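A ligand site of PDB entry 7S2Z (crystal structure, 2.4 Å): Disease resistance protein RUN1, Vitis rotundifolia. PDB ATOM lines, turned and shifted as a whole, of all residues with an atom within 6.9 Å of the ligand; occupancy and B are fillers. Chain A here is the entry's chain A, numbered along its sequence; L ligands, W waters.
The side-chain amide nitrogen (ND2) of Asn 145 lies within hydrogen-bond range of the backbone carbonyl oxygen (O) of Thr 141 (3.2 Å).
The side-chain hydroxyl of Thr 141 sits at hydrogen-bond distance from the backbone carbonyl oxygen of Arg 112, at 2.7 Å.
N of Phe 103 lies within hydrogen-bond range of O of Trp 149 (3.1 Å).
Merely in contact with the ligand: Pro 108, Pro 150 and Phe 103.
Hydrophobic or aromatic side chains within 4 Å of the ligand: Phe 103, Pro 108 and Pro 150.
Within 4 Å of the ligand: Phe 103, Pro 108, Arg 112, Ala 144, Asn 145, Leu 146, Ser 147, Gly 148 and Pro 150.
The nearest printed residue that does not touch the ligand is Trp 149 (4.5 Å).
A nitrogen (N7) of the ligand lies within hydrogen-bond range of the backbone carbonyl oxygen of Asn 145.
OD1 of Asn 145 sits at hydrogen-bond distance from O13 of the ligand (2.5 Å).
A nitrogen (N3) of the ligand is in hydrogen-bond range of the backbone carbonyl oxygen of Leu 146.
A nitrogen (N4) of the ligand lies within hydrogen-bond range of the backbone NH (N) of Gly 148 (2.9 Å).
The backbone carbonyl oxygen of Ala 144 is in hydrogen-bond range of a nitrogen (N3) of the ligand, 2.9 Å away.
An oxygen (O1) of the ligand lies within salt-bridge range of the guanidinium group of Arg 112.
The side-chain hydroxyl of Ser 147 is in hydrogen-bond range of an oxygen (O14) of the ligand (3.2 Å).
Water W1 lies within hydrogen-bond range of O of Ala 144, N2 of the ligand and NE of Arg 112.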
ATOM      1  N   PRO A 101     -23.832 -17.632 -23.443  1.00  0.00           N
ATOM      2  CA  PRO A 101     -24.981 -17.442 -24.327  1.00  0.00           C
ATOM      3  C   PRO A 101     -26.280 -17.986 -23.738  1.00  0.00           C
ATOM      4  O   PRO A 101     -26.322 -19.078 -23.176  1.00  0.00           O
ATOM      5  CB  PRO A 101     -24.586 -18.225 -25.578  1.00  0.00           C
ATOM      6  CG  PRO A 101     -23.770 -19.358 -25.048  1.00  0.00           C
ATOM      7  CD  PRO A 101     -23.085 -18.857 -23.783  1.00  0.00           C
ATOM      8  N   PHE A 103     -30.112 -18.796 -24.999  1.00  0.00           N
ATOM      9  CA  PHE A 103     -30.997 -18.985 -26.146  1.00  0.00           C
ATOM     10  C   PHE A 103     -32.430 -18.825 -25.641  1.00  0.00           C
ATOM     11  O   PHE A 103     -33.081 -19.794 -25.243  1.00  0.00           O
ATOM     12  CB  PHE A 103     -30.759 -20.351 -26.797  1.00  0.00           C
ATOM     13  CG  PHE A 103     -29.320 -20.636 -27.088  1.00  0.00           C
ATOM     14  CD1 PHE A 103     -28.735 -20.197 -28.270  1.00  0.00           C
ATOM     15  CD2 PHE A 103     -28.543 -21.344 -26.188  1.00  0.00           C
ATOM     16  CE1 PHE A 103     -27.400 -20.459 -28.538  1.00  0.00           C
ATOM     17  CE2 PHE A 103     -27.207 -21.606 -26.456  1.00  0.00           C
ATOM     18  CZ  PHE A 103     -26.642 -21.165 -27.628  1.00  0.00           C
ATOM     19  N   ASP A 107     -34.212 -21.905 -30.815  1.00  0.00           N
ATOM     20  CA  ASP A 107     -33.460 -23.145 -30.910  1.00  0.00           C
ATOM     21  C   ASP A 107     -31.968 -22.824 -31.030  1.00  0.00           C
ATOM     22  O   ASP A 107     -31.576 -22.038 -31.892  1.00  0.00           O
ATOM     23  CB  ASP A 107     -33.929 -23.954 -32.129  1.00  0.00           C
ATOM     24  CG  ASP A 107     -33.621 -25.432 -31.996  1.00  0.00           C
ATOM     25  OD1 ASP A 107     -32.529 -25.774 -31.501  1.00  0.00           O
ATOM     26  OD2 ASP A 107     -34.489 -26.247 -32.394  1.00  0.00           O
ATOM     27  N   PRO A 108     -31.120 -23.403 -30.168  1.00  0.00           N
ATOM     28  CA  PRO A 108     -29.680 -23.126 -30.308  1.00  0.00           C
ATOM     29  C   PRO A 108     -29.139 -23.385 -31.700  1.00  0.00           C
ATOM     30  O   PRO A 108     -28.249 -22.667 -32.167  1.00  0.00           O
ATOM     31  CB  PRO A 108     -29.053 -24.073 -29.273  1.00  0.00           C
ATOM     32  CG  PRO A 108     -30.118 -24.301 -28.272  1.00  0.00           C
ATOM     33  CD  PRO A 108     -31.421 -24.248 -29.010  1.00  0.00           C
ATOM     34  N   SER A 109     -29.654 -24.410 -32.391  1.00  0.00           N
ATOM     35  CA  SER A 109     -29.184 -24.711 -33.735  1.00  0.00           C
ATOM     36  C   SER A 109     -29.630 -23.664 -34.751  1.00  0.00           C
ATOM     37  O   SER A 109     -28.972 -23.515 -35.781  1.00  0.00           O
ATOM     38  CB  SER A 109     -29.670 -26.096 -34.156  1.00  0.00           C
ATOM     39  OG  SER A 109     -31.007 -26.055 -34.626  1.00  0.00           O
ATOM     40  N   ARG A 112     -26.756 -21.244 -34.312  1.00  0.00           N
ATOM     41  CA  ARG A 112     -25.494 -21.809 -34.761  1.00  0.00           C
ATOM     42  C   ARG A 112     -25.433 -21.918 -36.278  1.00  0.00           C
ATOM     43  O   ARG A 112     -24.393 -21.656 -36.895  1.00  0.00           O
ATOM     44  CB  ARG A 112     -25.291 -23.189 -34.125  1.00  0.00           C
ATOM     45  CG  ARG A 112     -23.949 -23.829 -34.411  1.00  0.00           C
ATOM     46  CD  ARG A 112     -23.995 -25.337 -34.160  1.00  0.00           C
ATOM     47  NE  ARG A 112     -24.977 -25.683 -33.144  1.00  0.00           N
ATOM     48  CZ  ARG A 112     -25.990 -26.531 -33.310  1.00  0.00           C
ATOM     49  NH1 ARG A 112     -26.158 -27.188 -34.448  1.00  0.00           N
ATOM     50  NH2 ARG A 112     -26.837 -26.723 -32.315  1.00  0.00           N
ATOM     51  N   THR A 141     -22.121 -18.472 -35.091  1.00  0.00           N
ATOM     52  CA  THR A 141     -21.797 -19.895 -34.977  1.00  0.00           C
ATOM     53  C   THR A 141     -20.835 -20.153 -33.820  1.00  0.00           C
ATOM     54  O   THR A 141     -21.027 -21.097 -33.052  1.00  0.00           O
ATOM     55  CB  THR A 141     -21.185 -20.392 -36.293  1.00  0.00           C
ATOM     56  OG1 THR A 141     -22.146 -20.281 -37.347  1.00  0.00           O
ATOM     57  CG2 THR A 141     -20.753 -21.844 -36.156  1.00  0.00           C
ATOM     58  N   ALA A 143     -20.371 -18.253 -31.088  1.00  0.00           N
ATOM     59  CA  ALA A 143     -21.031 -17.987 -29.814  1.00  0.00           C
ATOM     60  C   ALA A 143     -21.967 -19.120 -29.422  1.00  0.00           C
ATOM     61  O   ALA A 143     -22.101 -19.453 -28.241  1.00  0.00           O
ATOM     62  CB  ALA A 143     -21.788 -16.660 -29.881  1.00  0.00           C
ATOM     63  N   ALA A 144     -22.647 -19.718 -30.407  1.00  0.00           N
ATOM     64  CA  ALA A 144     -23.592 -20.786 -30.124  1.00  0.00           C
ATOM     65  C   ALA A 144     -22.904 -22.092 -29.750  1.00  0.00           C
ATOM     66  O   ALA A 144     -23.593 -23.034 -29.333  1.00  0.00           O
ATOM     67  CB  ALA A 144     -24.497 -21.018 -31.335  1.00  0.00           C
ATOM     68  N   ASN A 145     -21.582 -22.183 -29.884  1.00  0.00           N
ATOM     69  CA  ASN A 145     -20.838 -23.377 -29.548  1.00  0.00           C
ATOM     70  C   ASN A 145     -20.190 -23.305 -28.162  1.00  0.00           C
ATOM     71  O   ASN A 145     -19.422 -24.193 -27.804  1.00  0.00           O
ATOM     72  CB  ASN A 145     -19.766 -23.651 -30.607  1.00  0.00           C
ATOM     73  CG  ASN A 145     -20.266 -24.551 -31.711  1.00  0.00           C
ATOM     74  OD1 ASN A 145     -20.848 -25.603 -31.458  1.00  0.00           O
ATOM     75  ND2 ASN A 145     -20.034 -24.141 -32.962  1.00  0.00           N
ATOM     76  N   LEU A 146     -20.500 -22.267 -27.385  1.00  0.00           N
ATOM     77  CA  LEU A 146     -20.078 -22.182 -25.996  1.00  0.00           C
ATOM     78  C   LEU A 146     -21.219 -22.657 -25.101  1.00  0.00           C
ATOM     79  O   LEU A 146     -22.393 -22.419 -25.404  1.00  0.00           O
ATOM     80  CB  LEU A 146     -19.684 -20.755 -25.609  1.00  0.00           C
ATOM     81  CG  LEU A 146     -18.452 -20.155 -26.307  1.00  0.00           C
ATOM     82  CD1 LEU A 146     -18.782 -19.813 -27.732  1.00  0.00           C
ATOM     83  CD2 LEU A 146     -17.996 -18.919 -25.578  1.00  0.00           C
ATOM     84  N   SER A 147     -20.862 -23.303 -23.998  1.00  0.00           N
ATOM     85  CA  SER A 147     -21.872 -23.831 -23.079  1.00  0.00           C
ATOM     86  C   SER A 147     -22.744 -22.701 -22.570  1.00  0.00           C
ATOM     87  O   SER A 147     -22.245 -21.760 -21.927  1.00  0.00           O
ATOM     88  CB  SER A 147     -21.187 -24.552 -21.924  1.00  0.00           C
ATOM     89  OG  SER A 147     -20.756 -25.838 -22.315  1.00  0.00           O
ATOM     90  N   GLY A 148     -24.044 -22.783 -22.845  1.00  0.00           N
ATOM     91  CA  GLY A 148     -25.010 -21.786 -22.447  1.00  0.00           C
ATOM     92  C   GLY A 148     -26.241 -22.429 -21.848  1.00  0.00           C
ATOM     93  O   GLY A 148     -26.175 -23.479 -21.205  1.00  0.00           O
ATOM     94  N   TRP A 149     -27.381 -21.781 -22.069  1.00  0.00           N
ATOM     95  CA  TRP A 149     -28.656 -22.208 -21.488  1.00  0.00           C
ATOM     96  C   TRP A 149     -29.752 -22.082 -22.546  1.00  0.00           C
ATOM     97  O   TRP A 149     -30.215 -20.966 -22.837  1.00  0.00           O
ATOM     98  CB  TRP A 149     -29.007 -21.384 -20.257  1.00  0.00           C
ATOM     99  CG  TRP A 149     -28.050 -21.548 -19.135  1.00  0.00           C
ATOM    100  CD1 TRP A 149     -28.113 -22.460 -18.120  1.00  0.00           C
ATOM    101  CD2 TRP A 149     -26.859 -20.777 -18.898  1.00  0.00           C
ATOM    102  NE1 TRP A 149     -27.047 -22.306 -17.273  1.00  0.00           N
ATOM    103  CE2 TRP A 149     -26.264 -21.280 -17.723  1.00  0.00           C
ATOM    104  CE3 TRP A 149     -26.250 -19.714 -19.567  1.00  0.00           C
ATOM    105  CZ2 TRP A 149     -25.082 -20.755 -17.210  1.00  0.00           C
ATOM    106  CZ3 TRP A 149     -25.084 -19.194 -19.056  1.00  0.00           C
ATOM    107  CH2 TRP A 149     -24.515 -19.712 -17.886  1.00  0.00           C
ATOM    108  N   PRO A 150     -30.193 -23.190 -23.128  1.00  0.00           N
ATOM    109  CA  PRO A 150     -31.408 -23.149 -23.963  1.00  0.00           C
ATOM    110  C   PRO A 150     -32.635 -22.967 -23.068  1.00  0.00           C
ATOM    111  O   PRO A 150     -32.894 -23.783 -22.186  1.00  0.00           O
ATOM    112  CB  PRO A 150     -31.413 -24.506 -24.671  1.00  0.00           C
ATOM    113  CG  PRO A 150     -30.055 -25.103 -24.422  1.00  0.00           C
ATOM    114  CD  PRO A 150     -29.583 -24.528 -23.136  1.00  0.00           C
HETATM  115  P1  LIG L   1     -28.235 -31.172 -30.338  1.00  0.00           P
HETATM  116  O1  LIG L   1     -27.991 -30.181 -31.413  1.00  0.00           O
HETATM  117  O2  LIG L   1     -29.677 -31.654 -30.236  1.00  0.00           O
HETATM  118  O3  LIG L   1     -27.829 -30.579 -28.864  1.00  0.00           O
HETATM  119  C1  LIG L   1     -27.969 -31.381 -27.679  1.00  0.00           C
HETATM  120  C2  LIG L   1     -28.641 -30.568 -26.608  1.00  0.00           C
HETATM  121  O4  LIG L   1     -27.790 -29.465 -26.221  1.00  0.00           O
HETATM  122  C3  LIG L   1     -29.984 -29.944 -26.998  1.00  0.00           C
HETATM  123  O5  LIG L   1     -30.913 -30.012 -25.914  1.00  0.00           O
HETATM  124  C4  LIG L   1     -29.612 -28.508 -27.337  1.00  0.00           C
HETATM  125  O6  LIG L   1     -30.702 -27.609 -27.109  1.00  0.00           O
HETATM  126  C5  LIG L   1     -28.497 -28.248 -26.324  1.00  0.00           C
HETATM  127  N1  LIG L   1     -27.555 -27.209 -26.706  1.00  0.00           N
HETATM  128  C6  LIG L   1     -27.229 -26.788 -27.967  1.00  0.00           C
HETATM  129  N2  LIG L   1     -26.336 -25.838 -28.002  1.00  0.00           N
HETATM  130  C7  LIG L   1     -26.047 -25.597 -26.676  1.00  0.00           C
HETATM  131  C8  LIG L   1     -25.163 -24.708 -26.030  1.00  0.00           C
HETATM  132  N3  LIG L   1     -24.374 -23.853 -26.680  1.00  0.00           N
HETATM  133  N4  LIG L   1     -25.126 -24.717 -24.681  1.00  0.00           N
HETATM  134  C9  LIG L   1     -25.906 -25.584 -24.022  1.00  0.00           C
HETATM  135  N5  LIG L   1     -26.770 -26.477 -24.516  1.00  0.00           N
HETATM  136  C10 LIG L   1     -26.793 -26.434 -25.854  1.00  0.00           C
HETATM  137  O7  LIG L   1     -27.325 -32.471 -30.506  1.00  0.00           O
HETATM  138  P2  LIG L   1     -25.742 -32.735 -30.533  1.00  0.00           P
HETATM  139  O8  LIG L   1     -25.436 -33.646 -31.655  1.00  0.00           O
HETATM  140  O9  LIG L   1     -25.296 -33.089 -29.175  1.00  0.00           O
HETATM  141  O10 LIG L   1     -25.187 -31.273 -30.855  1.00  0.00           O
HETATM  142  C11 LIG L   1     -25.012 -30.840 -32.228  1.00  0.00           C
HETATM  143  C12 LIG L   1     -24.081 -29.661 -32.238  1.00  0.00           C
HETATM  144  O11 LIG L   1     -24.606 -28.616 -31.406  1.00  0.00           O
HETATM  145  C13 LIG L   1     -22.676 -29.926 -31.716  1.00  0.00           C
HETATM  146  O12 LIG L   1     -21.838 -30.431 -32.743  1.00  0.00           O
HETATM  147  C14 LIG L   1     -22.238 -28.532 -31.245  1.00  0.00           C
HETATM  148  O13 LIG L   1     -21.736 -27.743 -32.313  1.00  0.00           O
HETATM  149  C15 LIG L   1     -23.562 -27.954 -30.727  1.00  0.00           C
HETATM  150  N6  LIG L   1     -23.753 -28.181 -29.223  1.00  0.00           N
HETATM  151  C16 LIG L   1     -22.957 -27.455 -28.419  1.00  0.00           C
HETATM  152  C17 LIG L   1     -23.056 -27.589 -27.042  1.00  0.00           C
HETATM  153  C18 LIG L   1     -22.169 -26.782 -26.140  1.00  0.00           C
HETATM  154  O14 LIG L   1     -22.262 -26.921 -24.906  1.00  0.00           O
HETATM  155  N7  LIG L   1     -21.317 -25.941 -26.697  1.00  0.00           N
HETATM  156  C19 LIG L   1     -23.987 -28.480 -26.524  1.00  0.00           C
HETATM  157  C20 LIG L   1     -24.790 -29.215 -27.382  1.00  0.00           C
HETATM  158  C21 LIG L   1     -24.663 -29.051 -28.744  1.00  0.00           C
HETATM  159  O   HOH W   1     -25.024 -24.946 -30.312  1.00  0.00           O
